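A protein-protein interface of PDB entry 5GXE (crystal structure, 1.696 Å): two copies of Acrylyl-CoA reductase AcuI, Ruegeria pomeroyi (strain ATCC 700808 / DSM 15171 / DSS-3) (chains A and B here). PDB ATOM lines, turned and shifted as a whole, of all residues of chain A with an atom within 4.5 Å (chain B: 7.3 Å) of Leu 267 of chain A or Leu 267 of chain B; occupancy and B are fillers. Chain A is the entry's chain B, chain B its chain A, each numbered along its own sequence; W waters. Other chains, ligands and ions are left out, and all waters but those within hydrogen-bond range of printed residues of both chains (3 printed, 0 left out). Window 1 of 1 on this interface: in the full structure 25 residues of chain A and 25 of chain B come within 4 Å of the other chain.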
ATOM      1  N   LEU A 229      -5.733  -0.637 -21.114  1.00  0.00           N
ATOM      2  CA  LEU A 229      -5.501  -1.468 -22.292  1.00  0.00           C
ATOM      3  C   LEU A 229      -6.715  -1.461 -23.214  1.00  0.00           C
ATOM      4  O   LEU A 229      -6.576  -1.334 -24.436  1.00  0.00           O
ATOM      5  CB  LEU A 229      -5.153  -2.900 -21.872  1.00  0.00           C
ATOM      6  CG  LEU A 229      -5.021  -3.955 -22.983  1.00  0.00           C
ATOM      7  CD1 LEU A 229      -4.029  -3.539 -24.046  1.00  0.00           C
ATOM      8  CD2 LEU A 229      -4.632  -5.312 -22.388  1.00  0.00           C
ATOM      9  N   VAL A 242      -0.354  -4.596 -29.733  1.00  0.00           N
ATOM     10  CA  VAL A 242      -0.071  -4.325 -28.329  1.00  0.00           C
ATOM     11  C   VAL A 242       0.562  -5.570 -27.736  1.00  0.00           C
ATOM     12  O   VAL A 242      -0.013  -6.660 -27.815  1.00  0.00           O
ATOM     13  CB  VAL A 242      -1.332  -3.945 -27.534  1.00  0.00           C
ATOM     14  CG1 VAL A 242      -0.967  -3.703 -26.053  1.00  0.00           C
ATOM     15  CG2 VAL A 242      -2.016  -2.715 -28.127  1.00  0.00           C
ATOM     16  N   ALA A 244       0.970  -7.368 -24.566  1.00  0.00           N
ATOM     17  CA  ALA A 244       0.358  -7.390 -23.242  1.00  0.00           C
ATOM     18  C   ALA A 244       1.330  -8.013 -22.251  1.00  0.00           C
ATOM     19  O   ALA A 244       1.686  -9.184 -22.392  1.00  0.00           O
ATOM     20  CB  ALA A 244      -0.958  -8.166 -23.284  1.00  0.00           C
ATOM     21  N   LEU A 253     -10.368  -6.963 -18.720  1.00  0.00           N
ATOM     22  CA  LEU A 253     -10.135  -6.330 -20.019  1.00  0.00           C
ATOM     23  C   LEU A 253     -11.479  -5.948 -20.628  1.00  0.00           C
ATOM     24  O   LEU A 253     -12.084  -6.735 -21.377  1.00  0.00           O
ATOM     25  CB  LEU A 253      -9.346  -7.257 -20.942  1.00  0.00           C
ATOM     26  CG  LEU A 253      -9.052  -6.787 -22.364  1.00  0.00           C
ATOM     27  CD1 LEU A 253      -8.467  -5.401 -22.333  1.00  0.00           C
ATOM     28  CD2 LEU A 253      -8.099  -7.756 -23.048  1.00  0.00           C
ATOM     29  N   PHE A 260      -9.891  -5.052 -33.515  1.00  0.00           N
ATOM     30  CA  PHE A 260      -9.321  -6.223 -34.165  1.00  0.00           C
ATOM     31  C   PHE A 260      -9.921  -6.416 -35.553  1.00  0.00           C
ATOM     32  O   PHE A 260      -9.195  -6.615 -36.531  1.00  0.00           O
ATOM     33  CB  PHE A 260      -9.536  -7.462 -33.282  1.00  0.00           C
ATOM     34  CG  PHE A 260      -8.946  -7.323 -31.906  1.00  0.00           C
ATOM     35  CD1 PHE A 260      -7.636  -7.704 -31.658  1.00  0.00           C
ATOM     36  CD2 PHE A 260      -9.689  -6.769 -30.871  1.00  0.00           C
ATOM     37  CE1 PHE A 260      -7.080  -7.548 -30.389  1.00  0.00           C
ATOM     38  CE2 PHE A 260      -9.144  -6.617 -29.607  1.00  0.00           C
ATOM     39  CZ  PHE A 260      -7.839  -7.008 -29.363  1.00  0.00           C
ATOM     40  N   VAL A 265      -5.888  -4.946 -35.633  1.00  0.00           N
ATOM     41  CA  VAL A 265      -5.034  -4.824 -34.449  1.00  0.00           C
ATOM     42  C   VAL A 265      -4.766  -6.207 -33.867  1.00  0.00           C
ATOM     43  O   VAL A 265      -5.603  -7.112 -33.958  1.00  0.00           O
ATOM     44  CB  VAL A 265      -5.701  -3.893 -33.417  1.00  0.00           C
ATOM     45  CG1 VAL A 265      -4.962  -3.867 -32.080  1.00  0.00           C
ATOM     46  CG2 VAL A 265      -5.753  -2.458 -33.973  1.00  0.00           C
ATOM     47  N   ASN A 266      -3.584  -6.377 -33.274  1.00  0.00           N
ATOM     48  CA  ASN A 266      -3.242  -7.601 -32.551  1.00  0.00           C
ATOM     49  C   ASN A 266      -3.016  -7.307 -31.077  1.00  0.00           C
ATOM     50  O   ASN A 266      -2.458  -6.264 -30.720  1.00  0.00           O
ATOM     51  CB  ASN A 266      -1.984  -8.253 -33.106  1.00  0.00           C
ATOM     52  CG  ASN A 266      -2.085  -8.548 -34.572  1.00  0.00           C
ATOM     53  OD1 ASN A 266      -3.055  -9.145 -35.029  1.00  0.00           O
ATOM     54  ND2 ASN A 266      -1.071  -8.127 -35.329  1.00  0.00           N
ATOM     55  N   LEU A 267      -3.434  -8.246 -30.227  1.00  0.00           N
ATOM     56  CA  LEU A 267      -3.082  -8.242 -28.808  1.00  0.00           C
ATOM     57  C   LEU A 267      -2.215  -9.470 -28.573  1.00  0.00           C
ATOM     58  O   LEU A 267      -2.701 -10.606 -28.672  1.00  0.00           O
ATOM     59  CB  LEU A 267      -4.324  -8.249 -27.916  1.00  0.00           C
ATOM     60  CG  LEU A 267      -4.063  -8.113 -26.408  1.00  0.00           C
ATOM     61  CD1 LEU A 267      -3.262  -6.850 -26.085  1.00  0.00           C
ATOM     62  CD2 LEU A 267      -5.397  -8.118 -25.660  1.00  0.00           C
ATOM     63  N   LEU A 268      -0.943  -9.240 -28.247  1.00  0.00           N
ATOM     64  CA  LEU A 268       0.075 -10.289 -28.176  1.00  0.00           C
ATOM     65  C   LEU A 268       0.445 -10.553 -26.722  1.00  0.00           C
ATOM     66  O   LEU A 268       1.006  -9.674 -26.054  1.00  0.00           O
ATOM     67  CB  LEU A 268       1.318  -9.882 -28.966  1.00  0.00           C
ATOM     68  CG  LEU A 268       1.038  -9.489 -30.422  1.00  0.00           C
ATOM     69  CD1 LEU A 268       2.297  -8.951 -31.081  1.00  0.00           C
ATOM     70  CD2 LEU A 268       0.477 -10.667 -31.207  1.00  0.00           C
ATOM     71  N   GLY A 269       0.161 -11.764 -26.246  1.00  0.00           N
ATOM     72  CA  GLY A 269       0.424 -12.093 -24.856  1.00  0.00           C
ATOM     73  C   GLY A 269       1.887 -12.416 -24.655  1.00  0.00           C
ATOM     74  O   GLY A 269       2.459 -13.243 -25.374  1.00  0.00           O
ATOM     75  N   ASP B 222     -12.658 -17.293 -35.123  1.00  0.00           N
ATOM     76  CA  ASP B 222     -13.806 -16.825 -34.349  1.00  0.00           C
ATOM     77  C   ASP B 222     -14.672 -15.901 -35.186  1.00  0.00           C
ATOM     78  O   ASP B 222     -14.270 -14.770 -35.478  1.00  0.00           O
ATOM     79  CB  ASP B 222     -13.376 -16.095 -33.080  1.00  0.00           C
ATOM     80  CG  ASP B 222     -14.561 -15.552 -32.319  1.00  0.00           C
ATOM     81  OD1 ASP B 222     -15.622 -16.223 -32.348  1.00  0.00           O
ATOM     82  OD2 ASP B 222     -14.443 -14.471 -31.702  1.00  0.00           O
ATOM     83  N   LEU B 229     -16.055 -15.300 -27.292  1.00  0.00           N
ATOM     84  CA  LEU B 229     -14.624 -15.068 -27.482  1.00  0.00           C
ATOM     85  C   LEU B 229     -13.911 -14.896 -26.145  1.00  0.00           C
ATOM     86  O   LEU B 229     -12.828 -15.455 -25.937  1.00  0.00           O
ATOM     87  CB  LEU B 229     -14.395 -13.842 -28.373  1.00  0.00           C
ATOM     88  CG  LEU B 229     -12.941 -13.349 -28.482  1.00  0.00           C
ATOM     89  CD1 LEU B 229     -11.997 -14.451 -28.942  1.00  0.00           C
ATOM     90  CD2 LEU B 229     -12.876 -12.163 -29.445  1.00  0.00           C
ATOM     91  N   LEU B 233     -10.816 -17.464 -24.873  1.00  0.00           N
ATOM     92  CA  LEU B 233      -9.449 -17.040 -24.584  1.00  0.00           C
ATOM     93  C   LEU B 233      -8.873 -17.795 -23.388  1.00  0.00           C
ATOM     94  O   LEU B 233      -7.694 -18.161 -23.394  1.00  0.00           O
ATOM     95  CB  LEU B 233      -9.399 -15.530 -24.343  1.00  0.00           C
ATOM     96  CG  LEU B 233      -9.579 -14.705 -25.624  1.00  0.00           C
ATOM     97  CD1 LEU B 233      -9.813 -13.243 -25.297  1.00  0.00           C
ATOM     98  CD2 LEU B 233      -8.364 -14.845 -26.530  1.00  0.00           C
ATOM     99  N   ALA B 240      -1.036 -20.349 -28.158  1.00  0.00           N
ATOM    100  CA  ALA B 240      -2.026 -20.451 -29.226  1.00  0.00           C
ATOM    101  C   ALA B 240      -2.670 -19.093 -29.514  1.00  0.00           C
ATOM    102  O   ALA B 240      -2.645 -18.172 -28.692  1.00  0.00           O
ATOM    103  CB  ALA B 240      -3.105 -21.475 -28.860  1.00  0.00           C
ATOM    104  N   SER B 241      -3.260 -18.983 -30.701  1.00  0.00           N
ATOM    105  CA  SER B 241      -3.832 -17.732 -31.182  1.00  0.00           C
ATOM    106  C   SER B 241      -5.292 -17.914 -31.577  1.00  0.00           C
ATOM    107  O   SER B 241      -5.705 -18.983 -32.043  1.00  0.00           O
ATOM    108  CB  SER B 241      -3.058 -17.201 -32.394  1.00  0.00           C
ATOM    109  OG  SER B 241      -1.698 -16.994 -32.081  1.00  0.00           O
ATOM    110  N   VAL B 242      -6.069 -16.863 -31.347  1.00  0.00           N
ATOM    111  CA  VAL B 242      -7.419 -16.717 -31.900  1.00  0.00           C
ATOM    112  C   VAL B 242      -7.360 -15.717 -33.041  1.00  0.00           C
ATOM    113  O   VAL B 242      -6.874 -14.593 -32.868  1.00  0.00           O
ATOM    114  CB  VAL B 242      -8.420 -16.244 -30.828  1.00  0.00           C
ATOM    115  CG1 VAL B 242      -9.821 -16.084 -31.424  1.00  0.00           C
ATOM    116  CG2 VAL B 242      -8.432 -17.212 -29.632  1.00  0.00           C
ATOM    117  N   ALA B 243      -7.864 -16.118 -34.203  1.00  0.00           N
ATOM    118  CA  ALA B 243      -8.064 -15.198 -35.314  1.00  0.00           C
ATOM    119  C   ALA B 243      -9.452 -14.593 -35.164  1.00  0.00           C
ATOM    120  O   ALA B 243     -10.460 -15.285 -35.354  1.00  0.00           O
ATOM    121  CB  ALA B 243      -7.904 -15.922 -36.649  1.00  0.00           C
ATOM    122  N   ALA B 244      -9.505 -13.309 -34.808  1.00  0.00           N
ATOM    123  CA  ALA B 244     -10.773 -12.612 -34.608  1.00  0.00           C
ATOM    124  C   ALA B 244     -11.330 -12.169 -35.954  1.00  0.00           C
ATOM    125  O   ALA B 244     -10.717 -11.344 -36.644  1.00  0.00           O
ATOM    126  CB  ALA B 244     -10.589 -11.407 -33.687  1.00  0.00           C
ATOM    127  N   VAL B 245     -12.479 -12.730 -36.330  1.00  0.00           N
ATOM    128  CA  VAL B 245     -13.116 -12.445 -37.607  1.00  0.00           C
ATOM    129  C   VAL B 245     -14.436 -11.705 -37.427  1.00  0.00           C
ATOM    130  O   VAL B 245     -14.709 -10.750 -38.156  1.00  0.00           O
ATOM    131  CB  VAL B 245     -13.322 -13.748 -38.413  1.00  0.00           C
ATOM    132  CG1 VAL B 245     -14.227 -13.509 -39.652  1.00  0.00           C
ATOM    133  CG2 VAL B 245     -11.987 -14.341 -38.820  1.00  0.00           C
ATOM    134  N   LEU B 253     -16.233  -7.317 -25.684  1.00  0.00           N
ATOM    135  CA  LEU B 253     -15.261  -8.364 -25.378  1.00  0.00           C
ATOM    136  C   LEU B 253     -15.004  -8.322 -23.880  1.00  0.00           C
ATOM    137  O   LEU B 253     -14.076  -7.647 -23.413  1.00  0.00           O
ATOM    138  CB  LEU B 253     -13.977  -8.181 -26.184  1.00  0.00           C
ATOM    139  CG  LEU B 253     -12.861  -9.200 -25.942  1.00  0.00           C
ATOM    140  CD1 LEU B 253     -13.412 -10.614 -26.092  1.00  0.00           C
ATOM    141  CD2 LEU B 253     -11.727  -8.946 -26.915  1.00  0.00           C
ATOM    142  N   ALA B 255     -13.386  -9.654 -21.475  1.00  0.00           N
ATOM    143  CA  ALA B 255     -12.257 -10.549 -21.281  1.00  0.00           C
ATOM    144  C   ALA B 255     -11.474 -10.174 -20.026  1.00  0.00           C
ATOM    145  O   ALA B 255     -11.807  -9.223 -19.312  1.00  0.00           O
ATOM    146  CB  ALA B 255     -11.354 -10.524 -22.521  1.00  0.00           C
ATOM    147  N   THR B 256     -10.439 -10.969 -19.740  1.00  0.00           N
ATOM    148  CA  THR B 256      -9.365 -10.611 -18.822  1.00  0.00           C
ATOM    149  C   THR B 256      -8.045 -10.727 -19.568  1.00  0.00           C
ATOM    150  O   THR B 256      -7.948 -11.418 -20.584  1.00  0.00           O
ATOM    151  CB  THR B 256      -9.306 -11.512 -17.564  1.00  0.00           C
ATOM    152  OG1 THR B 256      -8.669 -12.755 -17.886  1.00  0.00           O
ATOM    153  CG2 THR B 256     -10.689 -11.794 -17.024  1.00  0.00           C
ATOM    154  N   VAL B 257      -7.014 -10.052 -19.053  1.00  0.00           N
ATOM    155  CA  VAL B 257      -5.698 -10.150 -19.686  1.00  0.00           C
ATOM    156  C   VAL B 257      -4.956 -11.425 -19.311  1.00  0.00           C
ATOM    157  O   VAL B 257      -3.916 -11.719 -19.915  1.00  0.00           O
ATOM    158  CB  VAL B 257      -4.776  -8.968 -19.330  1.00  0.00           C
ATOM    159  CG1 VAL B 257      -5.413  -7.655 -19.705  1.00  0.00           C
ATOM    160  CG2 VAL B 257      -4.419  -8.995 -17.848  1.00  0.00           C
ATOM    161  N   PHE B 260      -3.502 -13.912 -21.886  1.00  0.00           N
ATOM    162  CA  PHE B 260      -2.395 -13.305 -22.612  1.00  0.00           C
ATOM    163  C   PHE B 260      -1.117 -13.352 -21.789  1.00  0.00           C
ATOM    164  O   PHE B 260      -0.058 -13.748 -22.283  1.00  0.00           O
ATOM    165  CB  PHE B 260      -2.763 -11.871 -22.976  1.00  0.00           C
ATOM    166  CG  PHE B 260      -4.000 -11.786 -23.839  1.00  0.00           C
ATOM    167  CD1 PHE B 260      -3.910 -11.870 -25.224  1.00  0.00           C
ATOM    168  CD2 PHE B 260      -5.253 -11.664 -23.257  1.00  0.00           C
ATOM    169  CE1 PHE B 260      -5.043 -11.821 -26.007  1.00  0.00           C
ATOM    170  CE2 PHE B 260      -6.396 -11.605 -24.031  1.00  0.00           C
ATOM    171  CZ  PHE B 260      -6.296 -11.690 -25.418  1.00  0.00           C
ATOM    172  N   GLY B 264       0.751 -16.603 -22.967  1.00  0.00           N
ATOM    173  CA  GLY B 264       1.217 -16.130 -24.254  1.00  0.00           C
ATOM    174  C   GLY B 264       0.196 -16.268 -25.364  1.00  0.00           C
ATOM    175  O   GLY B 264       0.576 -16.442 -26.526  1.00  0.00           O
ATOM    176  N   VAL B 265      -1.101 -16.202 -25.035  1.00  0.00           N
ATOM    177  CA  VAL B 265      -2.147 -16.277 -26.052  1.00  0.00           C
ATOM    178  C   VAL B 265      -2.159 -14.990 -26.882  1.00  0.00           C
ATOM    179  O   VAL B 265      -1.811 -13.907 -26.397  1.00  0.00           O
ATOM    180  CB  VAL B 265      -3.507 -16.538 -25.374  1.00  0.00           C
ATOM    181  CG1 VAL B 265      -4.684 -16.445 -26.375  1.00  0.00           C
ATOM    182  CG2 VAL B 265      -3.498 -17.907 -24.680  1.00  0.00           C
ATOM    183  N   ASN B 266      -2.528 -15.113 -28.151  1.00  0.00           N
ATOM    184  CA  ASN B 266      -2.661 -13.966 -29.047  1.00  0.00           C
ATOM    185  C   ASN B 266      -4.088 -13.837 -29.554  1.00  0.00           C
ATOM    186  O   ASN B 266      -4.745 -14.836 -29.857  1.00  0.00           O
ATOM    187  CB  ASN B 266      -1.745 -14.091 -30.259  1.00  0.00           C
ATOM    188  CG  ASN B 266      -0.311 -14.305 -29.879  1.00  0.00           C
ATOM    189  OD1 ASN B 266       0.259 -13.518 -29.129  1.00  0.00           O
ATOM    190  ND2 ASN B 266       0.294 -15.362 -30.418  1.00  0.00           N
ATOM    191  N   LEU B 267      -4.554 -12.600 -29.664  1.00  0.00           N
ATOM    192  CA  LEU B 267      -5.791 -12.282 -30.368  1.00  0.00           C
ATOM    193  C   LEU B 267      -5.421 -11.485 -31.612  1.00  0.00           C
ATOM    194  O   LEU B 267      -4.902 -10.366 -31.509  1.00  0.00           O
ATOM    195  CB  LEU B 267      -6.747 -11.501 -29.463  1.00  0.00           C
ATOM    196  CG  LEU B 267      -8.116 -11.144 -30.051  1.00  0.00           C
ATOM    197  CD1 LEU B 267      -8.857 -12.408 -30.520  1.00  0.00           C
ATOM    198  CD2 LEU B 267      -8.923 -10.399 -28.995  1.00  0.00           C
ATOM    199  N   LEU B 268      -5.674 -12.068 -32.789  1.00  0.00           N
ATOM    200  CA  LEU B 268      -5.166 -11.544 -34.051  1.00  0.00           C
ATOM    201  C   LEU B 268      -6.350 -11.022 -34.843  1.00  0.00           C
ATOM    202  O   LEU B 268      -7.227 -11.803 -35.221  1.00  0.00           O
ATOM    203  CB  LEU B 268      -4.448 -12.640 -34.836  1.00  0.00           C
ATOM    204  CG  LEU B 268      -3.325 -13.359 -34.097  1.00  0.00           C
ATOM    205  CD1 LEU B 268      -2.824 -14.480 -34.978  1.00  0.00           C
ATOM    206  CD2 LEU B 268      -2.202 -12.396 -33.727  1.00  0.00           C
ATOM    207  N   GLY B 269      -6.377  -9.715 -35.095  1.00  0.00           N
ATOM    208  CA  GLY B 269      -7.496  -9.119 -35.814  1.00  0.00           C
ATOM    209  C   GLY B 269      -7.380  -9.365 -37.303  1.00  0.00           C
ATOM    210  O   GLY B 269      -6.345  -9.076 -37.915  1.00  0.00           O
ATOM    211  N   ILE B 270      -8.457  -9.879 -37.900  1.00  0.00           N
ATOM    212  CA  ILE B 270      -8.499 -10.174 -39.327  1.00  0.00           C
ATOM    213  C   ILE B 270      -9.384  -9.136 -40.004  1.00  0.00           C
ATOM    214  O   ILE B 270     -10.563  -9.005 -39.658  1.00  0.00           O
ATOM    215  CB  ILE B 270      -9.038 -11.584 -39.598  1.00  0.00           C
ATOM    216  CG1 ILE B 270      -8.265 -12.618 -38.780  1.00  0.00           C
ATOM    217  CG2 ILE B 270      -8.978 -11.899 -41.093  1.00  0.00           C
ATOM    218  CD1 ILE B 270      -6.773 -12.653 -39.072  1.00  0.00           C
HETATM  219  O   HOH W   1      -3.744  -9.746 -37.545  1.00  0.00           O
HETATM  220  O   HOH W   2     -13.966  -7.528 -18.727  1.00  0.00           O
HETATM  221  O   HOH W   3       2.816 -13.411 -28.069  1.00  0.00           O
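The backbone carbonyl oxygen (O) of Ala 255 of chain B sits at hydrogen-bond distance from the backbone NH (N) of Leu 253 of chain A (2.7 Å).
The backbone carbonyl oxygen of Val 265 of chain B is in hydrogen-bond range of the backbone NH of Gly 269 of chain A, at 2.9 Å.
OD1 of Asn 266 of chain B is in hydrogen-bond range of N of Gly 269 of chain A, at 3.4 Å.
O of Leu 267 of chain B lies within hydrogen-bond range of N of Leu 267 of chain A (2.9 Å).
The backbone carbonyl oxygen of Val 265 of chain A lies within hydrogen-bond range of the backbone NH of Gly 269 of chain B (2.9 Å).
The side-chain amide oxygen (OD1) of Asn 266 of chain A sits at hydrogen-bond distance from the backbone NH (N) of Gly 269 of chain B (3.4 Å).
The backbone carbonyl oxygen of Leu 253 of chain B lies close to the backbone carbonyl oxygen of Leu 253 of chain A, at 3.0 Å.
O of Ala 240 of chain B is in hydrogen-bond range of N of Asn 266 of chain B.
The side-chain amide nitrogen of Asn 266 of chain B is in hydrogen-bond range of the side-chain hydroxyl of Ser 241 of chain B (3.1 Å).
The backbone carbonyl oxygen (O) of Val 242 of chain B is in hydrogen-bond range of the backbone NH (N) of Leu 268 of chain B, at 2.8 Å.
The backbone carbonyl oxygen (O) of Leu 268 of chain B is in hydrogen-bond range of the backbone NH (N) of Ala 244 of chain B (2.8 Å).
The backbone carbonyl oxygen (O) of Ala 244 of chain B lies within hydrogen-bond range of the backbone NH (N) of Ile 270 of chain B (3.0 Å).
The backbone NH (N) of Val 242 of chain A is in hydrogen-bond range of the backbone carbonyl oxygen (O) of Asn 266 of chain A, 2.9 Å away.
Among the printed residues, merely in contact across the chains: Gly 269 of chain A with Phe 260 of chain B, Phe 260 of chain A with Gly 269 of chain B, Gly 269 of chain A with Gly 264 of chain B, Asn 266 of chain A with Leu 268 of chain B, Leu 268 of chain A with Asn 266 of chain B, Leu 267 of chain A with Asn 266 of chain B, Asn 266 of chain A with Leu 267 of chain B, Phe 260 of chain A with Leu 267 of chain B, Phe 260 of chain A with Ile 270 of chain B, Leu 229 of chain A with Val 257 of chain B, Leu 267 of chain A with Phe 260 of chain B and Leu 253 of chain A with Thr 256 of chain B.
Printed residues of chain B within 4 Å of Leu 267 of chain A: Phe 260, Asn 266 and Leu 267.
Leu 267 of chain B touches three residues of chain A.
Of the printed residues of chain B, Gly 269 of chain A touches Phe 260 (3.1 Å), Gly 264 (3.3 Å), Val 265 (2.9 Å) and Asn 266 (3.4 Å).
Of the printed residues of chain A, Leu 253 of chain B touches Leu 253 (3.0 Å).
Of the printed residues of chain A, Val 257 of chain B touches Leu 229 (3.6 Å).
Of the printed residues of chain A, Leu 268 of chain B touches Asn 266.
Of the printed residues of chain B, Leu 229 of chain A touches Val 257.
The nearest printed residue of chain B that does not touch Val 265 of chain A is Leu 268 of chain B (4.1 Å).
Hydrophobic or aromatic side chains of chain B within 4 Å of the printed part of chain A: Val 257, Phe 260, Leu 267 and Leu 268.
Along chain A the printed residues that touch a printed residue of chain B span positions 229 to 269.
Leu 253 of chain B touches its own counterpart, Leu 253 of chain A.
Asn 266 of chain A touches Leu 267 of chain B, and with the chains exchanged Leu 267 of chain A touches Asn 266 of chain B.
Asn 266 of chain A touches Leu 268 of chain B, and with the chains exchanged Leu 268 of chain A touches Asn 266 of chain B.
Asn 266 of chain A touches Gly 269 of chain B, and with the chains exchanged Gly 269 of chain A touches Asn 266 of chain B.
Positions printed for both chains: 229, 242, 244, 253, 260, 265, 266, 267, 268 and 269.
Of the 19 pairs that touch across the chains among the printed residues, 14 have their exchanged pair printed and touching as well.
Water W1 lies within hydrogen-bond range of OD1 of Asn 266 of chain A (2.7 Å) and O of Gly 269 of chain B (2.7 Å).
Water W3 lies within hydrogen-bond range of the backbone carbonyl oxygen (O) of Gly 269 of chain A (2.7 Å) and the side-chain amide oxygen (OD1) of Asn 266 of chain B (2.8 Å).
Water W2 lies within hydrogen-bond range of the backbone carbonyl oxygen of Ala 255 of chain B and the backbone carbonyl oxygen of Leu 253 of chain A.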
